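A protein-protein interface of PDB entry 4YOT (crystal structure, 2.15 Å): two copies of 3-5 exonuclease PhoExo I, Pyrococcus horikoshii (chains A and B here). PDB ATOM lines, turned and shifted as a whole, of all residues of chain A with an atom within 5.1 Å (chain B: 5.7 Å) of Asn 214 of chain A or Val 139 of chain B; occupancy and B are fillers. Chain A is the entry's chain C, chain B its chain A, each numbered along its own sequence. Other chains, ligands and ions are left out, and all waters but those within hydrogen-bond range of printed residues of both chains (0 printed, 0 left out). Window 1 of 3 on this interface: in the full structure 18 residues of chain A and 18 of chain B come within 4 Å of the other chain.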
ATOM      1  N   LEU A  13      15.998 -21.667  12.132  1.00  0.00           N
ATOM      2  CA  LEU A  13      15.373 -20.590  11.370  1.00  0.00           C
ATOM      3  C   LEU A  13      14.231 -21.155  10.529  1.00  0.00           C
ATOM      4  O   LEU A  13      14.273 -22.322  10.136  1.00  0.00           O
ATOM      5  CB  LEU A  13      16.387 -19.922  10.443  1.00  0.00           C
ATOM      6  CG  LEU A  13      17.772 -19.555  10.985  1.00  0.00           C
ATOM      7  CD1 LEU A  13      18.631 -18.969   9.884  1.00  0.00           C
ATOM      8  CD2 LEU A  13      17.648 -18.574  12.126  1.00  0.00           C
ATOM      9  N   PHE A  17      14.422 -17.267   7.114  1.00  0.00           N
ATOM     10  CA  PHE A  17      15.586 -16.927   7.943  1.00  0.00           C
ATOM     11  C   PHE A  17      15.252 -16.239   9.258  1.00  0.00           C
ATOM     12  O   PHE A  17      16.147 -15.743   9.949  1.00  0.00           O
ATOM     13  CB  PHE A  17      16.614 -16.106   7.158  1.00  0.00           C
ATOM     14  CG  PHE A  17      16.948 -16.694   5.830  1.00  0.00           C
ATOM     15  CD1 PHE A  17      17.659 -17.884   5.743  1.00  0.00           C
ATOM     16  CD2 PHE A  17      16.541 -16.066   4.665  1.00  0.00           C
ATOM     17  CE1 PHE A  17      17.957 -18.435   4.514  1.00  0.00           C
ATOM     18  CE2 PHE A  17      16.836 -16.607   3.433  1.00  0.00           C
ATOM     19  CZ  PHE A  17      17.547 -17.793   3.355  1.00  0.00           C
ATOM     20  N   TYR A 212      26.013 -21.202   3.959  1.00  0.00           N
ATOM     21  CA  TYR A 212      25.942 -19.966   3.184  1.00  0.00           C
ATOM     22  C   TYR A 212      25.562 -18.779   4.072  1.00  0.00           C
ATOM     23  O   TYR A 212      25.050 -18.970   5.177  1.00  0.00           O
ATOM     24  CB  TYR A 212      24.969 -20.112   2.001  1.00  0.00           C
ATOM     25  CG  TYR A 212      23.548 -20.493   2.375  1.00  0.00           C
ATOM     26  CD1 TYR A 212      22.647 -19.536   2.825  1.00  0.00           C
ATOM     27  CD2 TYR A 212      23.102 -21.809   2.256  1.00  0.00           C
ATOM     28  CE1 TYR A 212      21.353 -19.872   3.158  1.00  0.00           C
ATOM     29  CE2 TYR A 212      21.801 -22.158   2.586  1.00  0.00           C
ATOM     30  CZ  TYR A 212      20.933 -21.181   3.035  1.00  0.00           C
ATOM     31  OH  TYR A 212      19.639 -21.502   3.369  1.00  0.00           O
ATOM     32  N   PRO A 213      25.840 -17.548   3.605  1.00  0.00           N
ATOM     33  CA  PRO A 213      25.460 -16.360   4.376  1.00  0.00           C
ATOM     34  C   PRO A 213      23.957 -16.228   4.612  1.00  0.00           C
ATOM     35  O   PRO A 213      23.154 -16.436   3.703  1.00  0.00           O
ATOM     36  CB  PRO A 213      25.921 -15.206   3.480  1.00  0.00           C
ATOM     37  CG  PRO A 213      27.072 -15.773   2.703  1.00  0.00           C
ATOM     38  CD  PRO A 213      26.682 -17.206   2.441  1.00  0.00           C
ATOM     39  N   ASN A 214      23.585 -15.887   5.837  1.00  0.00           N
ATOM     40  CA  ASN A 214      22.231 -15.431   6.108  1.00  0.00           C
ATOM     41  C   ASN A 214      22.083 -14.075   5.421  1.00  0.00           C
ATOM     42  O   ASN A 214      22.752 -13.116   5.801  1.00  0.00           O
ATOM     43  CB  ASN A 214      22.037 -15.286   7.615  1.00  0.00           C
ATOM     44  CG  ASN A 214      20.607 -14.960   7.999  1.00  0.00           C
ATOM     45  OD1 ASN A 214      19.903 -14.231   7.291  1.00  0.00           O
ATOM     46  ND2 ASN A 214      20.171 -15.494   9.133  1.00  0.00           N
ATOM     47  N   PRO A 215      21.210 -13.989   4.404  1.00  0.00           N
ATOM     48  CA  PRO A 215      21.171 -12.750   3.613  1.00  0.00           C
ATOM     49  C   PRO A 215      20.628 -11.579   4.414  1.00  0.00           C
ATOM     50  O   PRO A 215      20.807 -10.424   4.024  1.00  0.00           O
ATOM     51  CB  PRO A 215      20.204 -13.090   2.477  1.00  0.00           C
ATOM     52  CG  PRO A 215      19.321 -14.182   3.037  1.00  0.00           C
ATOM     53  CD  PRO A 215      20.224 -14.985   3.939  1.00  0.00           C
ATOM     54  N   LEU A 216      19.974 -11.881   5.529  1.00  0.00           N
ATOM     55  CA  LEU A 216      19.317 -10.857   6.329  1.00  0.00           C
ATOM     56  C   LEU A 216      20.176 -10.420   7.515  1.00  0.00           C
ATOM     57  O   LEU A 216      19.874  -9.428   8.177  1.00  0.00           O
ATOM     58  CB  LEU A 216      17.957 -11.367   6.816  1.00  0.00           C
ATOM     59  CG  LEU A 216      16.725 -11.116   5.940  1.00  0.00           C
ATOM     60  CD1 LEU A 216      17.021 -11.243   4.458  1.00  0.00           C
ATOM     61  CD2 LEU A 216      15.606 -12.067   6.327  1.00  0.00           C
ATOM     62  N   VAL A 217      21.237 -11.172   7.796  1.00  0.00           N
ATOM     63  CA  VAL A 217      22.077 -10.895   8.957  1.00  0.00           C
ATOM     64  C   VAL A 217      23.560 -11.024   8.593  1.00  0.00           C
ATOM     65  O   VAL A 217      24.143 -12.108   8.686  1.00  0.00           O
ATOM     66  CB  VAL A 217      21.740 -11.825  10.162  1.00  0.00           C
ATOM     67  CG1 VAL A 217      22.365 -11.281  11.426  1.00  0.00           C
ATOM     68  CG2 VAL A 217      20.233 -11.953  10.360  1.00  0.00           C
ATOM     69  N   ARG A 218      24.161  -9.908   8.188  1.00  0.00           N
ATOM     70  CA  ARG A 218      25.550  -9.871   7.734  1.00  0.00           C
ATOM     71  C   ARG A 218      26.500 -10.451   8.780  1.00  0.00           C
ATOM     72  O   ARG A 218      26.326 -10.202   9.971  1.00  0.00           O
ATOM     73  CB  ARG A 218      25.942  -8.427   7.404  1.00  0.00           C
ATOM     74  CG  ARG A 218      27.184  -8.278   6.539  1.00  0.00           C
ATOM     75  CD  ARG A 218      27.466  -6.808   6.220  1.00  0.00           C
ATOM     76  NE  ARG A 218      26.408  -6.209   5.411  1.00  0.00           N
ATOM     77  CZ  ARG A 218      26.334  -4.912   5.114  1.00  0.00           C
ATOM     78  NH1 ARG A 218      27.255  -4.069   5.570  1.00  0.00           N
ATOM     79  NH2 ARG A 218      25.327  -4.455   4.374  1.00  0.00           N
ATOM     80  N   PHE A 220      26.689 -13.536   9.661  1.00  0.00           N
ATOM     81  CA  PHE A 220      26.117 -14.752  10.246  1.00  0.00           C
ATOM     82  C   PHE A 220      25.872 -15.779   9.147  1.00  0.00           C
ATOM     83  O   PHE A 220      25.313 -15.450   8.094  1.00  0.00           O
ATOM     84  CB  PHE A 220      24.789 -14.454  10.952  1.00  0.00           C
ATOM     85  CG  PHE A 220      24.935 -13.752  12.279  1.00  0.00           C
ATOM     86  CD1 PHE A 220      25.402 -12.445  12.347  1.00  0.00           C
ATOM     87  CD2 PHE A 220      24.571 -14.393  13.460  1.00  0.00           C
ATOM     88  CE1 PHE A 220      25.519 -11.795  13.567  1.00  0.00           C
ATOM     89  CE2 PHE A 220      24.686 -13.747  14.685  1.00  0.00           C
ATOM     90  CZ  PHE A 220      25.159 -12.447  14.736  1.00  0.00           C
ATOM     91  N   MET A 221      26.275 -17.022   9.390  1.00  0.00           N
ATOM     92  CA  MET A 221      26.110 -18.073   8.392  1.00  0.00           C
ATOM     93  C   MET A 221      24.908 -18.959   8.716  1.00  0.00           C
ATOM     94  O   MET A 221      24.438 -19.005   9.856  1.00  0.00           O
ATOM     95  CB  MET A 221      27.387 -18.916   8.274  1.00  0.00           C
ATOM     96  CG  MET A 221      28.650 -18.104   7.992  1.00  0.00           C
ATOM     97  SD  MET A 221      28.578 -17.157   6.449  1.00  0.00           S
ATOM     98  CE  MET A 221      28.814 -15.486   7.066  1.00  0.00           C
ATOM     99  N   VAL A 222      24.404 -19.644   7.697  1.00  0.00           N
ATOM    100  CA  VAL A 222      23.275 -20.545   7.846  1.00  0.00           C
ATOM    101  C   VAL A 222      23.770 -21.931   7.481  1.00  0.00           C
ATOM    102  O   VAL A 222      24.404 -22.098   6.436  1.00  0.00           O
ATOM    103  CB  VAL A 222      22.133 -20.174   6.876  1.00  0.00           C
ATOM    104  CG1 VAL A 222      21.101 -21.289   6.805  1.00  0.00           C
ATOM    105  CG2 VAL A 222      21.477 -18.845   7.273  1.00  0.00           C
ATOM    106  N   VAL B  30      20.019 -10.768  -5.857  1.00  0.00           N
ATOM    107  CA  VAL B  30      20.767 -11.777  -5.116  1.00  0.00           C
ATOM    108  C   VAL B  30      19.890 -12.978  -4.777  1.00  0.00           C
ATOM    109  O   VAL B  30      18.815 -12.830  -4.190  1.00  0.00           O
ATOM    110  CB  VAL B  30      21.368 -11.204  -3.820  1.00  0.00           C
ATOM    111  CG1 VAL B  30      22.138 -12.280  -3.073  1.00  0.00           C
ATOM    112  CG2 VAL B  30      22.271 -10.013  -4.127  1.00  0.00           C
ATOM    113  N   TYR B  34      23.587 -16.502  -1.922  1.00  0.00           N
ATOM    114  CA  TYR B  34      23.715 -15.152  -1.372  1.00  0.00           C
ATOM    115  C   TYR B  34      25.176 -14.714  -1.199  1.00  0.00           C
ATOM    116  O   TYR B  34      25.524 -14.100  -0.193  1.00  0.00           O
ATOM    117  CB  TYR B  34      22.966 -15.038  -0.031  1.00  0.00           C
ATOM    118  CG  TYR B  34      21.564 -15.629  -0.051  1.00  0.00           C
ATOM    119  CD1 TYR B  34      20.519 -14.967  -0.675  1.00  0.00           C
ATOM    120  CD2 TYR B  34      21.293 -16.846   0.566  1.00  0.00           C
ATOM    121  CE1 TYR B  34      19.240 -15.503  -0.692  1.00  0.00           C
ATOM    122  CE2 TYR B  34      20.021 -17.388   0.559  1.00  0.00           C
ATOM    123  CZ  TYR B  34      19.001 -16.716  -0.074  1.00  0.00           C
ATOM    124  OH  TYR B  34      17.734 -17.254  -0.089  1.00  0.00           O
ATOM    125  N   LYS B  35      26.021 -15.030  -2.178  1.00  0.00           N
ATOM    126  CA  LYS B  35      27.431 -14.646  -2.127  1.00  0.00           C
ATOM    127  C   LYS B  35      27.783 -13.663  -3.231  1.00  0.00           C
ATOM    128  O   LYS B  35      28.758 -12.919  -3.125  1.00  0.00           O
ATOM    129  CB  LYS B  35      28.329 -15.874  -2.246  1.00  0.00           C
ATOM    130  CG  LYS B  35      28.361 -16.748  -1.010  1.00  0.00           C
ATOM    131  CD  LYS B  35      29.110 -18.049  -1.292  1.00  0.00           C
ATOM    132  CE  LYS B  35      29.346 -18.836  -0.015  1.00  0.00           C
ATOM    133  NZ  LYS B  35      30.033 -20.144  -0.253  1.00  0.00           N
ATOM    134  N   HIS B  78      15.879  -4.498  -0.682  1.00  0.00           N
ATOM    135  CA  HIS B  78      16.651  -3.996   0.447  1.00  0.00           C
ATOM    136  C   HIS B  78      17.279  -2.650   0.115  1.00  0.00           C
ATOM    137  O   HIS B  78      18.032  -2.533  -0.856  1.00  0.00           O
ATOM    138  CB  HIS B  78      17.750  -4.985   0.829  1.00  0.00           C
ATOM    139  CG  HIS B  78      17.254  -6.167   1.597  1.00  0.00           C
ATOM    140  ND1 HIS B  78      18.101  -7.114   2.135  1.00  0.00           N
ATOM    141  CD2 HIS B  78      15.997  -6.561   1.920  1.00  0.00           C
ATOM    142  CE1 HIS B  78      17.386  -8.038   2.756  1.00  0.00           C
ATOM    143  NE2 HIS B  78      16.108  -7.725   2.639  1.00  0.00           N
ATOM    144  N   SER B 137      22.690  -4.506   7.772  1.00  0.00           N
ATOM    145  CA  SER B 137      22.396  -5.864   8.191  1.00  0.00           C
ATOM    146  C   SER B 137      22.266  -6.773   6.971  1.00  0.00           C
ATOM    147  O   SER B 137      22.252  -8.002   7.094  1.00  0.00           O
ATOM    148  CB  SER B 137      21.115  -5.881   9.025  1.00  0.00           C
ATOM    149  OG  SER B 137      20.799  -7.192   9.446  1.00  0.00           O
ATOM    150  N   SER B 138      22.198  -6.162   5.790  1.00  0.00           N
ATOM    151  CA  SER B 138      21.840  -6.887   4.572  1.00  0.00           C
ATOM    152  C   SER B 138      23.037  -7.337   3.745  1.00  0.00           C
ATOM    153  O   SER B 138      23.924  -6.545   3.437  1.00  0.00           O
ATOM    154  CB  SER B 138      20.902  -6.039   3.713  1.00  0.00           C
ATOM    155  OG  SER B 138      20.787  -6.562   2.401  1.00  0.00           O
ATOM    156  N   VAL B 139      23.059  -8.619   3.383  1.00  0.00           N
ATOM    157  CA  VAL B 139      24.100  -9.131   2.491  1.00  0.00           C
ATOM    158  C   VAL B 139      23.908  -8.625   1.047  1.00  0.00           C
ATOM    159  O   VAL B 139      24.867  -8.187   0.420  1.00  0.00           O
ATOM    160  CB  VAL B 139      24.228 -10.686   2.562  1.00  0.00           C
ATOM    161  CG1 VAL B 139      25.184 -11.214   1.503  1.00  0.00           C
ATOM    162  CG2 VAL B 139      24.688 -11.118   3.953  1.00  0.00           C
ATOM    163  N   PRO B 140      22.671  -8.677   0.517  1.00  0.00           N
ATOM    164  CA  PRO B 140      22.474  -8.076  -0.806  1.00  0.00           C
ATOM    165  C   PRO B 140      22.924  -6.611  -0.901  1.00  0.00           C
ATOM    166  O   PRO B 140      23.464  -6.223  -1.941  1.00  0.00           O
ATOM    167  CB  PRO B 140      20.966  -8.201  -1.006  1.00  0.00           C
ATOM    168  CG  PRO B 140      20.647  -9.525  -0.334  1.00  0.00           C
ATOM    169  CD  PRO B 140      21.508  -9.507   0.911  1.00  0.00           C
ATOM    170  N   VAL B 141      22.719  -5.815   0.144  1.00  0.00           N
ATOM    171  CA  VAL B 141      23.238  -4.450   0.133  1.00  0.00           C
ATOM    172  C   VAL B 141      24.772  -4.442   0.037  1.00  0.00           C
ATOM    173  O   VAL B 141      25.348  -3.657  -0.725  1.00  0.00           O
ATOM    174  CB  VAL B 141      22.761  -3.644   1.350  1.00  0.00           C
ATOM    175  CG1 VAL B 141      23.543  -2.330   1.477  1.00  0.00           C
ATOM    176  CG2 VAL B 141      21.276  -3.350   1.230  1.00  0.00           C
ATOM    177  N   ARG B 142      25.430  -5.323   0.788  1.00  0.00           N
ATOM    178  CA  ARG B 142      26.896  -5.414   0.753  1.00  0.00           C
ATOM    179  C   ARG B 142      27.380  -5.848  -0.631  1.00  0.00           C
ATOM    180  O   ARG B 142      28.390  -5.350  -1.137  1.00  0.00           O
ATOM    181  CB  ARG B 142      27.411  -6.372   1.837  1.00  0.00           C
ATOM    182  CG  ARG B 142      28.931  -6.624   1.808  1.00  0.00           C
ATOM    183  CD  ARG B 142      29.783  -5.349   1.890  1.00  0.00           C
ATOM    184  NE  ARG B 142      31.199  -5.687   2.091  1.00  0.00           N
ATOM    185  CZ  ARG B 142      32.218  -4.848   1.919  1.00  0.00           C
ATOM    186  NH1 ARG B 142      32.004  -3.594   1.536  1.00  0.00           N
ATOM    187  NH2 ARG B 142      33.460  -5.268   2.129  1.00  0.00           N
ATOM    188  N   ILE B 143      26.642  -6.765  -1.250  1.00  0.00           N
ATOM    189  CA  ILE B 143      26.974  -7.225  -2.594  1.00  0.00           C
ATOM    190  C   ILE B 143      26.819  -6.079  -3.602  1.00  0.00           C
ATOM    191  O   ILE B 143      27.667  -5.896  -4.477  1.00  0.00           O
ATOM    192  CB  ILE B 143      26.134  -8.459  -2.977  1.00  0.00           C
ATOM    193  CG1 ILE B 143      26.585  -9.666  -2.148  1.00  0.00           C
ATOM    194  CG2 ILE B 143      26.257  -8.785  -4.451  1.00  0.00           C
ATOM    195  CD1 ILE B 143      25.716 -10.910  -2.327  1.00  0.00           C
ATOM    196  N   ALA B 144      25.746  -5.306  -3.468  1.00  0.00           N
ATOM    197  CA  ALA B 144      25.576  -4.102  -4.275  1.00  0.00           C
ATOM    198  C   ALA B 144      26.778  -3.174  -4.104  1.00  0.00           C
ATOM    199  O   ALA B 144      27.313  -2.648  -5.076  1.00  0.00           O
ATOM    200  CB  ALA B 144      24.294  -3.384  -3.881  1.00  0.00           C
ATOM    201  N   GLU B 192      32.341 -12.135   6.397  1.00  0.00           N
ATOM    202  CA  GLU B 192      31.162 -11.979   5.553  1.00  0.00           C
ATOM    203  C   GLU B 192      30.856 -13.235   4.744  1.00  0.00           C
ATOM    204  O   GLU B 192      29.811 -13.321   4.091  1.00  0.00           O
ATOM    205  CB  GLU B 192      31.296 -10.742   4.651  1.00  0.00           C
ATOM    206  CG  GLU B 192      31.279  -9.449   5.447  1.00  0.00           C
ATOM    207  CD  GLU B 192      31.240  -8.188   4.586  1.00  0.00           C
ATOM    208  OE1 GLU B 192      30.667  -7.189   5.060  1.00  0.00           O
ATOM    209  OE2 GLU B 192      31.791  -8.181   3.461  1.00  0.00           O
ATOM    210  N   LEU B 195      31.917 -12.882   0.085  1.00  0.00           N
ATOM    211  CA  LEU B 195      31.132 -12.104  -0.869  1.00  0.00           C
ATOM    212  C   LEU B 195      32.016 -11.572  -2.007  1.00  0.00           C
ATOM    213  O   LEU B 195      33.134 -11.096  -1.774  1.00  0.00           O
ATOM    214  CB  LEU B 195      30.414 -10.956  -0.158  1.00  0.00           C
ATOM    215  CG  LEU B 195      29.634 -11.354   1.098  1.00  0.00           C
ATOM    216  CD1 LEU B 195      28.941 -10.151   1.683  1.00  0.00           C
ATOM    217  CD2 LEU B 195      28.627 -12.469   0.816  1.00  0.00           C
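No position is printed for both chains.
The guanidinium group (NH2) of Arg 218 of chain A lies within hydrogen-bond range of the backbone carbonyl oxygen (O) of Ser 138 of chain B, at 2.7 Å. The side-chain hydroxyl (OG) of Ser 137 of chain B lies within hydrogen-bond range of the backbone carbonyl oxygen (O) of Leu 216 of chain A, 2.7 Å away. The backbone carbonyl oxygen (O) of Pro 215 of chain A lies within hydrogen-bond range of the backbone NH (N) of Val 139 of chain B (3.0 Å). N of Arg 218 of chain A lies within hydrogen-bond range of O of Ser 137 of chain B, 2.9 Å away. The backbone carbonyl oxygen (O) of Ser 137 of chain B is in hydrogen-bond range of the backbone NH (N) of Val 217 of chain A, at 3.4 Å.
Of the 12 printed residues of chain A, 9 touch a printed residue of chain B. Hydrophobic or aromatic side chains of chain A that line the printed part of chain B: Phe 17, Tyr 212, Pro 213, Pro 215, Leu 216 and Met 221. Along chain A the printed residues that touch a printed residue of chain B span positions 17 to 221. Of the 14 printed residues of chain B, 9 touch a printed residue of chain A. Hydrophobic or aromatic side chains of chain B within 4 Å of the printed part of chain A: Tyr 34, His 78, Val 139 and Pro 140. Among the printed residues, 18 pairs touch across the chains. Among the printed residues, no Asp or Glu carboxylate lies within 4 Å of a Lys or Arg side-chain nitrogen of the other chain.
The side-chain hydroxyl (OG) of Ser 138 of chain B sits at hydrogen-bond distance from a ring nitrogen (ND1) of His 78 of chain B (2.8 Å). The backbone NH (N) of Leu 216 of chain A lies within hydrogen-bond range of the side-chain amide oxygen (OD1) of Asn 214 of chain A. The backbone NH (N) of Asn 214 of chain A is in hydrogen-bond range of the backbone carbonyl oxygen (O) of Phe 220 of chain A (2.9 Å). The backbone NH (N) of Val 141 of chain B sits at hydrogen-bond distance from the side-chain hydroxyl (OG) of Ser 138 of chain B, 3.1 Å away. N of Val 217 of chain A lies within hydrogen-bond range of OD1 of Asn 214 of chain A (3.4 Å). NE of Arg 142 of chain B lies within salt-bridge range of OE2 of Glu 192 of chain B (2.9 Å).
Asn 214 of chain A touches one residue of chain B. Val 139 of chain B touches just these residues of chain A: Asn 214 (3.3 Å) and Pro 215 (3.0 Å). Of the printed residues of chain A, Tyr 34 of chain B touches Phe 17, Tyr 212, Pro 213 and Pro 215. Of the printed residues of chain A, Glu 192 of chain B touches Pro 213, Arg 218 and Met 221. Of the printed residues of chain A, Pro 140 of chain B touches Pro 215. Printed residues of chain B within 4 Å of Leu 216 of chain A: His 78 (3.6 Å) and Ser 137 (2.7 Å). Of the printed residues of chain A, Ser 138 of chain B touches Pro 215 and Arg 218. Leu 13 of chain A touches none of the printed residues of chain B. Phe 220 of chain A touches none of the printed residues of chain B. The nearest residue of chain A that does not touch Val 139 of chain B is Arg 218 of chain A (4.1 Å).
Among the printed residues, pairs that only touch across the chains: Pro 215 of chain A with Pro 140 of chain B (3.3 Å), Asn 214 of chain A with Val 139 of chain B (3.3 Å), Arg 218 of chain A with Glu 192 of chain B (3.4 Å), Phe 17 of chain A with Tyr 34 of chain B (3.5 Å), Leu 216 of chain A with His 78 of chain B (3.6 Å), Pro 213 of chain A with Tyr 34 of chain B (3.7 Å), Pro 215 of chain A with Tyr 34 of chain B (3.7 Å), Arg 218 of chain A with Arg 142 of chain B (3.7 Å), Pro 215 of chain A with Ser 138 of chain B (3.7 Å), Tyr 212 of chain A with Tyr 34 of chain B (3.8 Å), Met 221 of chain A with Glu 192 of chain B (3.8 Å), Pro 213 of chain A with Lys 35 of chain B (3.9 Å) and Pro 213 of chain A with Glu 192 of chain B (3.9 Å).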
